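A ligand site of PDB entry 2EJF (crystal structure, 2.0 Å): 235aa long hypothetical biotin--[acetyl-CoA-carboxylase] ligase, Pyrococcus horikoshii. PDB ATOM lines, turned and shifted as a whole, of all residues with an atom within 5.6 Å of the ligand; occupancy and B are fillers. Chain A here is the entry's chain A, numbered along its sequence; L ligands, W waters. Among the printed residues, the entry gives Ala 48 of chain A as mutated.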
ATOM      1  N   THR A  20       4.234   4.476 -28.718  1.00  0.00           N
ATOM      2  CA  THR A  20       3.447   3.791 -27.702  1.00  0.00           C
ATOM      3  C   THR A  20       1.963   4.163 -27.877  1.00  0.00           C
ATOM      4  O   THR A  20       1.096   3.283 -27.990  1.00  0.00           O
ATOM      5  CB  THR A  20       3.920   4.185 -26.291  1.00  0.00           C
ATOM      6  OG1 THR A  20       4.065   5.616 -26.217  1.00  0.00           O
ATOM      7  CG2 THR A  20       5.255   3.526 -25.955  1.00  0.00           C
ATOM      8  N   SER A  21       1.697   5.465 -27.893  1.00  0.00           N
ATOM      9  CA  SER A  21       0.340   5.987 -28.038  1.00  0.00           C
ATOM     10  C   SER A  21       0.369   7.397 -28.576  1.00  0.00           C
ATOM     11  O   SER A  21       1.077   8.258 -28.027  1.00  0.00           O
ATOM     12  CB  SER A  21      -0.367   5.985 -26.678  1.00  0.00           C
ATOM     13  OG  SER A  21      -1.549   6.752 -26.736  1.00  0.00           O
ATOM     14  N   THR A  22      -0.398   7.664 -29.632  1.00  0.00           N
ATOM     15  CA  THR A  22      -0.454   9.023 -30.164  1.00  0.00           C
ATOM     16  C   THR A  22      -1.124   9.962 -29.145  1.00  0.00           C
ATOM     17  O   THR A  22      -0.787  11.145 -29.079  1.00  0.00           O
ATOM     18  CB  THR A  22      -1.245   9.104 -31.515  1.00  0.00           C
ATOM     19  OG1 THR A  22      -2.560   8.564 -31.342  1.00  0.00           O
ATOM     20  CG2 THR A  22      -0.521   8.332 -32.600  1.00  0.00           C
ATOM     21  N   ASN A  23      -2.079   9.435 -28.373  1.00  0.00           N
ATOM     22  CA  ASN A  23      -2.765  10.250 -27.355  1.00  0.00           C
ATOM     23  C   ASN A  23      -1.805  10.751 -26.269  1.00  0.00           C
ATOM     24  O   ASN A  23      -1.903  11.898 -25.820  1.00  0.00           O
ATOM     25  CB  ASN A  23      -3.897   9.458 -26.664  1.00  0.00           C
ATOM     26  CG  ASN A  23      -5.304   9.740 -27.243  1.00  0.00           C
ATOM     27  OD1 ASN A  23      -5.417  10.217 -28.375  1.00  0.00           O
ATOM     28  ND2 ASN A  23      -6.345   9.471 -26.478  1.00  0.00           N
ATOM     29  N   GLU A  24      -0.887   9.895 -25.828  1.00  0.00           N
ATOM     30  CA  GLU A  24       0.071  10.302 -24.796  1.00  0.00           C
ATOM     31  C   GLU A  24       0.977  11.421 -25.307  1.00  0.00           C
ATOM     32  O   GLU A  24       1.207  12.405 -24.612  1.00  0.00           O
ATOM     33  CB  GLU A  24       0.938   9.120 -24.374  1.00  0.00           C
ATOM     34  CG  GLU A  24       0.401   8.334 -23.199  1.00  0.00           C
ATOM     35  CD  GLU A  24       0.074   9.206 -21.999  1.00  0.00           C
ATOM     36  OE1 GLU A  24       0.937  10.021 -21.584  1.00  0.00           O
ATOM     37  OE2 GLU A  24      -1.050   9.079 -21.459  1.00  0.00           O
ATOM     38  N   GLN A  42       0.893   1.576 -33.196  1.00  0.00           N
ATOM     39  CA  GLN A  42       1.013   1.961 -31.786  1.00  0.00           C
ATOM     40  C   GLN A  42       1.215   0.672 -31.014  1.00  0.00           C
ATOM     41  O   GLN A  42       0.484  -0.314 -31.230  1.00  0.00           O
ATOM     42  CB  GLN A  42      -0.264   2.603 -31.260  1.00  0.00           C
ATOM     43  CG  GLN A  42      -0.583   3.986 -31.729  1.00  0.00           C
ATOM     44  CD  GLN A  42      -1.852   4.517 -31.080  1.00  0.00           C
ATOM     45  OE1 GLN A  42      -1.908   5.670 -30.650  1.00  0.00           O
ATOM     46  NE2 GLN A  42      -2.887   3.675 -31.011  1.00  0.00           N
ATOM     47  N   MET A  44       1.330   0.646 -27.525  1.00  0.00           N
ATOM     48  CA  MET A  44       0.638   0.775 -26.243  1.00  0.00           C
ATOM     49  C   MET A  44      -0.677   1.530 -26.388  1.00  0.00           C
ATOM     50  O   MET A  44      -1.025   2.328 -25.519  1.00  0.00           O
ATOM     51  CB  MET A  44       1.533   1.507 -25.235  1.00  0.00           C
ATOM     52  CG  MET A  44       2.768   0.739 -24.769  1.00  0.00           C
ATOM     53  SD  MET A  44       2.339  -0.792 -23.915  1.00  0.00           S
ATOM     54  CE  MET A  44       3.463  -1.961 -24.697  1.00  0.00           C
ATOM     55  N   GLY A  45      -1.407   1.268 -27.476  1.00  0.00           N
ATOM     56  CA  GLY A  45      -2.674   1.933 -27.714  1.00  0.00           C
ATOM     57  C   GLY A  45      -3.635   1.936 -26.527  1.00  0.00           C
ATOM     58  O   GLY A  45      -3.863   0.923 -25.882  1.00  0.00           O
ATOM     59  N   HIS A  46      -4.225   3.107 -26.264  1.00  0.00           N
ATOM     60  CA  HIS A  46      -5.167   3.250 -25.167  1.00  0.00           C
ATOM     61  C   HIS A  46      -6.610   3.132 -25.605  1.00  0.00           C
ATOM     62  O   HIS A  46      -7.035   3.778 -26.572  1.00  0.00           O
ATOM     63  CB  HIS A  46      -5.011   4.620 -24.500  1.00  0.00           C
ATOM     64  CG  HIS A  46      -3.629   4.916 -24.029  1.00  0.00           C
ATOM     65  ND1 HIS A  46      -3.219   6.201 -23.719  1.00  0.00           N
ATOM     66  CD2 HIS A  46      -2.557   4.109 -23.817  1.00  0.00           C
ATOM     67  CE1 HIS A  46      -1.951   6.161 -23.343  1.00  0.00           C
ATOM     68  NE2 HIS A  46      -1.534   4.917 -23.386  1.00  0.00           N
ATOM     69  N   GLY A  47      -7.361   2.291 -24.907  1.00  0.00           N
ATOM     70  CA  GLY A  47      -8.771   2.158 -25.202  1.00  0.00           C
ATOM     71  C   GLY A  47      -9.443   2.960 -24.105  1.00  0.00           C
ATOM     72  O   GLY A  47      -8.751   3.451 -23.199  1.00  0.00           O
ATOM     73  N   ALA A  48     -10.762   3.107 -24.145  1.00  0.00           N
ATOM     74  CA  ALA A  48     -11.450   3.867 -23.108  1.00  0.00           C
ATOM     75  C   ALA A  48     -11.703   2.974 -21.899  1.00  0.00           C
ATOM     76  O   ALA A  48     -11.673   1.742 -22.001  1.00  0.00           O
ATOM     77  CB  ALA A  48     -12.766   4.412 -23.647  1.00  0.00           C
ATOM     78  N   ARG A  51      -9.331  -0.010 -21.061  1.00  0.00           N
ATOM     79  CA  ARG A  51      -9.182  -1.107 -22.035  1.00  0.00           C
ATOM     80  C   ARG A  51      -7.920  -0.853 -22.865  1.00  0.00           C
ATOM     81  O   ARG A  51      -7.360   0.235 -22.846  1.00  0.00           O
ATOM     82  CB  ARG A  51     -10.354  -1.137 -23.026  1.00  0.00           C
ATOM     83  CG  ARG A  51     -11.720  -1.530 -22.487  1.00  0.00           C
ATOM     84  CD  ARG A  51     -12.752  -1.414 -23.625  1.00  0.00           C
ATOM     85  NE  ARG A  51     -13.469  -0.134 -23.620  1.00  0.00           N
ATOM     86  CZ  ARG A  51     -14.530   0.111 -22.859  1.00  0.00           C
ATOM     87  NH1 ARG A  51     -15.004  -0.828 -22.049  1.00  0.00           N
ATOM     88  NH2 ARG A  51     -15.121   1.305 -22.887  1.00  0.00           N
ATOM     89  N   TRP A  53      -6.078  -0.916 -26.731  1.00  0.00           N
ATOM     90  CA  TRP A  53      -6.477  -0.828 -28.128  1.00  0.00           C
ATOM     91  C   TRP A  53      -5.377  -1.350 -29.057  1.00  0.00           C
ATOM     92  O   TRP A  53      -4.262  -0.824 -29.045  1.00  0.00           O
ATOM     93  CB  TRP A  53      -6.827   0.615 -28.504  1.00  0.00           C
ATOM     94  CG  TRP A  53      -7.338   0.764 -29.905  1.00  0.00           C
ATOM     95  CD1 TRP A  53      -6.619   1.113 -30.999  1.00  0.00           C
ATOM     96  CD2 TRP A  53      -8.675   0.555 -30.348  1.00  0.00           C
ATOM     97  NE1 TRP A  53      -7.429   1.140 -32.113  1.00  0.00           N
ATOM     98  CE2 TRP A  53      -8.700   0.805 -31.735  1.00  0.00           C
ATOM     99  CE3 TRP A  53      -9.875   0.179 -29.705  1.00  0.00           C
ATOM    100  CZ2 TRP A  53      -9.872   0.692 -32.503  1.00  0.00           C
ATOM    101  CZ3 TRP A  53     -11.030   0.069 -30.472  1.00  0.00           C
ATOM    102  CH2 TRP A  53     -11.021   0.326 -31.856  1.00  0.00           C
ATOM    103  N   SER A  55      -3.299  -1.676 -32.276  1.00  0.00           N
ATOM    104  CA  SER A  55      -3.000  -0.737 -33.366  1.00  0.00           C
ATOM    105  C   SER A  55      -1.922  -1.191 -34.356  1.00  0.00           C
ATOM    106  O   SER A  55      -0.903  -0.498 -34.520  1.00  0.00           O
ATOM    107  CB  SER A  55      -2.569   0.603 -32.761  1.00  0.00           C
ATOM    108  OG  SER A  55      -3.497   1.059 -31.811  1.00  0.00           O
ATOM    109  N   LEU A  60      -5.609   3.430 -39.190  1.00  0.00           N
ATOM    110  CA  LEU A  60      -5.428   4.869 -38.993  1.00  0.00           C
ATOM    111  C   LEU A  60      -5.499   5.144 -37.487  1.00  0.00           C
ATOM    112  O   LEU A  60      -6.572   5.067 -36.885  1.00  0.00           O
ATOM    113  CB  LEU A  60      -6.523   5.629 -39.741  1.00  0.00           C
ATOM    114  CG  LEU A  60      -6.406   7.154 -39.863  1.00  0.00           C
ATOM    115  CD1 LEU A  60      -5.071   7.522 -40.470  1.00  0.00           C
ATOM    116  CD2 LEU A  60      -7.562   7.677 -40.733  1.00  0.00           C
ATOM    117  N   TRP A  61      -4.343   5.466 -36.901  1.00  0.00           N
ATOM    118  CA  TRP A  61      -4.216   5.726 -35.469  1.00  0.00           C
ATOM    119  C   TRP A  61      -3.773   7.173 -35.319  1.00  0.00           C
ATOM    120  O   TRP A  61      -2.633   7.516 -35.627  1.00  0.00           O
ATOM    121  CB  TRP A  61      -3.142   4.800 -34.872  1.00  0.00           C
ATOM    122  CG  TRP A  61      -3.166   3.420 -35.446  1.00  0.00           C
ATOM    123  CD1 TRP A  61      -2.152   2.770 -36.074  1.00  0.00           C
ATOM    124  CD2 TRP A  61      -4.291   2.526 -35.463  1.00  0.00           C
ATOM    125  NE1 TRP A  61      -2.561   1.514 -36.482  1.00  0.00           N
ATOM    126  CE2 TRP A  61      -3.876   1.342 -36.120  1.00  0.00           C
ATOM    127  CE3 TRP A  61      -5.611   2.612 -34.996  1.00  0.00           C
ATOM    128  CZ2 TRP A  61      -4.730   0.255 -36.320  1.00  0.00           C
ATOM    129  CZ3 TRP A  61      -6.469   1.516 -35.197  1.00  0.00           C
ATOM    130  CH2 TRP A  61      -6.018   0.360 -35.858  1.00  0.00           C
ATOM    131  N   LEU A  62      -4.676   8.026 -34.830  1.00  0.00           N
ATOM    132  CA  LEU A  62      -4.351   9.451 -34.702  1.00  0.00           C
ATOM    133  C   LEU A  62      -4.986  10.120 -33.503  1.00  0.00           C
ATOM    134  O   LEU A  62      -5.940   9.596 -32.909  1.00  0.00           O
ATOM    135  CB  LEU A  62      -4.776  10.187 -35.984  1.00  0.00           C
ATOM    136  CG  LEU A  62      -6.275  10.197 -36.348  1.00  0.00           C
ATOM    137  CD1 LEU A  62      -6.993  11.285 -35.565  1.00  0.00           C
ATOM    138  CD2 LEU A  62      -6.432  10.437 -37.835  1.00  0.00           C
ATOM    139  N   SER A  63      -4.459  11.285 -33.163  1.00  0.00           N
ATOM    140  CA  SER A  63      -4.931  12.086 -32.054  1.00  0.00           C
ATOM    141  C   SER A  63      -4.916  13.540 -32.519  1.00  0.00           C
ATOM    142  O   SER A  63      -4.014  13.934 -33.265  1.00  0.00           O
ATOM    143  CB  SER A  63      -4.014  11.927 -30.840  1.00  0.00           C
ATOM    144  OG  SER A  63      -3.999  10.591 -30.374  1.00  0.00           O
ATOM    145  N   ASN A 103     -18.863   6.097 -27.928  1.00  0.00           N
ATOM    146  CA  ASN A 103     -17.596   6.285 -28.655  1.00  0.00           C
ATOM    147  C   ASN A 103     -17.167   5.256 -29.693  1.00  0.00           C
ATOM    148  O   ASN A 103     -16.029   5.317 -30.164  1.00  0.00           O
ATOM    149  CB  ASN A 103     -16.467   6.377 -27.642  1.00  0.00           C
ATOM    150  CG  ASN A 103     -16.150   5.038 -27.015  1.00  0.00           C
ATOM    151  OD1 ASN A 103     -17.058   4.308 -26.577  1.00  0.00           O
ATOM    152  ND2 ASN A 103     -14.868   4.708 -26.943  1.00  0.00           N
ATOM    153  N   ASP A 104     -18.039   4.322 -30.058  1.00  0.00           N
ATOM    154  CA  ASP A 104     -17.644   3.325 -31.040  1.00  0.00           C
ATOM    155  C   ASP A 104     -18.492   3.338 -32.306  1.00  0.00           C
ATOM    156  O   ASP A 104     -19.647   3.736 -32.288  1.00  0.00           O
ATOM    157  CB  ASP A 104     -17.663   1.927 -30.423  1.00  0.00           C
ATOM    158  CG  ASP A 104     -16.632   1.770 -29.315  1.00  0.00           C
ATOM    159  OD1 ASP A 104     -15.538   2.359 -29.423  1.00  0.00           O
ATOM    160  OD2 ASP A 104     -16.908   1.049 -28.340  1.00  0.00           O
ATOM    161  N   ALA A 113     -14.166   1.086 -35.486  1.00  0.00           N
ATOM    162  CA  ALA A 113     -13.470   2.250 -34.958  1.00  0.00           C
ATOM    163  C   ALA A 113     -13.845   2.566 -33.512  1.00  0.00           C
ATOM    164  O   ALA A 113     -14.908   2.153 -33.025  1.00  0.00           O
ATOM    165  CB  ALA A 113     -13.729   3.485 -35.842  1.00  0.00           C
ATOM    166  N   GLY A 114     -12.972   3.288 -32.817  1.00  0.00           N
ATOM    167  CA  GLY A 114     -13.221   3.641 -31.432  1.00  0.00           C
ATOM    168  C   GLY A 114     -12.665   5.040 -31.164  1.00  0.00           C
ATOM    169  O   GLY A 114     -11.635   5.408 -31.726  1.00  0.00           O
ATOM    170  N   VAL A 115     -13.339   5.798 -30.318  1.00  0.00           N
ATOM    171  CA  VAL A 115     -12.904   7.157 -29.981  1.00  0.00           C
ATOM    172  C   VAL A 115     -12.627   7.291 -28.481  1.00  0.00           C
ATOM    173  O   VAL A 115     -13.348   6.722 -27.647  1.00  0.00           O
ATOM    174  CB  VAL A 115     -13.990   8.214 -30.373  1.00  0.00           C
ATOM    175  CG1 VAL A 115     -13.457   9.647 -30.126  1.00  0.00           C
ATOM    176  CG2 VAL A 115     -14.396   8.036 -31.841  1.00  0.00           C
ATOM    177  N   LEU A 116     -11.578   8.029 -28.144  1.00  0.00           N
ATOM    178  CA  LEU A 116     -11.165   8.266 -26.765  1.00  0.00           C
ATOM    179  C   LEU A 116     -10.734   9.720 -26.630  1.00  0.00           C
ATOM    180  O   LEU A 116      -9.829  10.176 -27.337  1.00  0.00           O
ATOM    181  CB  LEU A 116      -9.990   7.376 -26.359  1.00  0.00           C
ATOM    182  CG  LEU A 116      -9.378   7.712 -24.991  1.00  0.00           C
ATOM    183  CD1 LEU A 116     -10.426   7.530 -23.896  1.00  0.00           C
ATOM    184  CD2 LEU A 116      -8.168   6.818 -24.725  1.00  0.00           C
ATOM    185  N   GLY A 127      -8.765  11.297 -29.619  1.00  0.00           N
ATOM    186  CA  GLY A 127      -8.070  10.159 -30.185  1.00  0.00           C
ATOM    187  C   GLY A 127      -9.024   9.281 -30.963  1.00  0.00           C
ATOM    188  O   GLY A 127     -10.122   8.982 -30.480  1.00  0.00           O
ATOM    189  N   ILE A 128      -8.601   8.869 -32.149  1.00  0.00           N
ATOM    190  CA  ILE A 128      -9.427   8.029 -33.002  1.00  0.00           C
ATOM    191  C   ILE A 128      -8.658   6.895 -33.641  1.00  0.00           C
ATOM    192  O   ILE A 128      -7.618   7.121 -34.259  1.00  0.00           O
ATOM    193  CB  ILE A 128     -10.080   8.843 -34.131  1.00  0.00           C
ATOM    194  CG1 ILE A 128     -10.881  10.005 -33.549  1.00  0.00           C
ATOM    195  CG2 ILE A 128     -10.930   7.927 -35.010  1.00  0.00           C
ATOM    196  CD1 ILE A 128     -11.287  11.053 -34.572  1.00  0.00           C
ATOM    197  N   GLY A 129      -9.168   5.673 -33.486  1.00  0.00           N
ATOM    198  CA  GLY A 129      -8.540   4.522 -34.086  1.00  0.00           C
ATOM    199  C   GLY A 129      -9.514   3.911 -35.072  1.00  0.00           C
ATOM    200  O   GLY A 129     -10.607   3.508 -34.679  1.00  0.00           O
HETATM  201  C1  LIG L   1     -12.192   2.602 -27.581  1.00  0.00           C
HETATM  202  O1  LIG L   1     -13.080   2.222 -28.359  1.00  0.00           O
HETATM  203  O2  LIG L   1     -11.959   1.988 -26.498  1.00  0.00           O
HETATM  204  C2  LIG L   1     -11.344   3.820 -27.892  1.00  0.00           C
HETATM  205  C3  LIG L   1     -10.144   3.512 -28.768  1.00  0.00           C
HETATM  206  C4  LIG L   1      -9.354   4.769 -29.124  1.00  0.00           C
HETATM  207  C5  LIG L   1      -8.160   4.411 -30.017  1.00  0.00           C
HETATM  208  C6  LIG L   1      -7.258   5.562 -30.498  1.00  0.00           C
HETATM  209  S1  LIG L   1      -5.933   4.995 -31.549  1.00  0.00           S
HETATM  210  C7  LIG L   1      -5.343   6.735 -31.638  1.00  0.00           C
HETATM  211  C8  LIG L   1      -5.363   7.142 -30.129  1.00  0.00           C
HETATM  212  N1  LIG L   1      -4.134   6.752 -29.411  1.00  0.00           N
HETATM  213  C9  LIG L   1      -4.461   5.918 -28.388  1.00  0.00           C
HETATM  214  O3  LIG L   1      -3.632   5.402 -27.573  1.00  0.00           O
HETATM  215  N2  LIG L   1      -5.821   5.703 -28.335  1.00  0.00           N
HETATM  216  C10 LIG L   1      -6.521   6.434 -29.393  1.00  0.00           C
HETATM  217  O   HOH W   1     -13.479  -0.439 -27.807  1.00  0.00           O
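An oxygen (O3) of the ligand sits at hydrogen-bond distance from the side-chain hydroxyl of Ser 21, 2.6 Å away. OD1 of Asp 104 sits close to O1 of the ligand (2.7 Å). O3 of the ligand lies within hydrogen-bond range of N of His 46, 2.7 Å away. The backbone carbonyl oxygen of His 46 sits at hydrogen-bond distance from a nitrogen (N2) of the ligand, at 2.9 Å. The side-chain amide oxygen of Gln 42 sits at hydrogen-bond distance from a nitrogen (N1) of the ligand (2.8 Å). N of Ala 48 sits at hydrogen-bond distance from O2 of the ligand (2.9 Å). OG1 of Thr 22 is in hydrogen-bond range of N1 of the ligand, at 3.1 Å. ND2 of Asn 103 lies within hydrogen-bond range of O1 of the ligand, at 3.4 Å. The guanidinium group (NE) of Arg 51 is in salt-bridge range of an oxygen (O2) of the ligand, 3.9 Å away.
The backbone NH (N) of Asn 23 lies within hydrogen-bond range of the side-chain hydroxyl (OG) of Ser 21 (3.2 Å). OG of Ser 21 sits at hydrogen-bond distance from N of Glu 24, at 3.3 Å. The side-chain amide oxygen (OE1) of Gln 42 sits at hydrogen-bond distance from the backbone NH (N) of Thr 22 (2.7 Å). The side-chain amide nitrogen (NE2) of Gln 42 sits at hydrogen-bond distance from the side-chain hydroxyl (OG) of Ser 55 (2.8 Å). N of Ile 128 lies within hydrogen-bond range of O of Leu 62, 2.9 Å away. The backbone NH (N) of Gly 114 sits at hydrogen-bond distance from the backbone carbonyl oxygen (O) of Gly 129, at 3.0 Å. The backbone carbonyl oxygen (O) of Trp 53 lies close to the side-chain hydroxyl (OG) of Ser 55. The backbone carbonyl oxygen (O) of Thr 20 is in hydrogen-bond range of the backbone NH (N) of Gly 45, at 3.3 Å.
Asn 23 touches the ligand (N to N1, 3.5 Å). Gly 45 touches the ligand. Gly 47 touches the ligand. Trp 53 touches the ligand. Leu 62 touches the ligand. Ser 63 touches the ligand. Gly 114 touches the ligand (CA to O1, 3.4 Å). O of Val 115 touches C2 of the ligand, 3.5 Å away. Leu 116 touches the ligand. Ile 128 touches the ligand. N of Gly 129 touches C6 of the ligand (3.5 Å). Hydrophobic or aromatic side chains within 4 Å of the ligand: His 46, Ala 48, Trp 53 and Leu 116. Within 4 Å of the ligand: Ser 21, Thr 22, Asn 23, Gln 42, Gly 45, His 46, Gly 47, Ala 48, Arg 51, Trp 53, Leu 62, Ser 63, Asn 103, Asp 104, Gly 114, Val 115, Leu 116, Ile 128 and Gly 129. Along chain A the residues within 4 Å of the ligand span positions 21 to 129.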
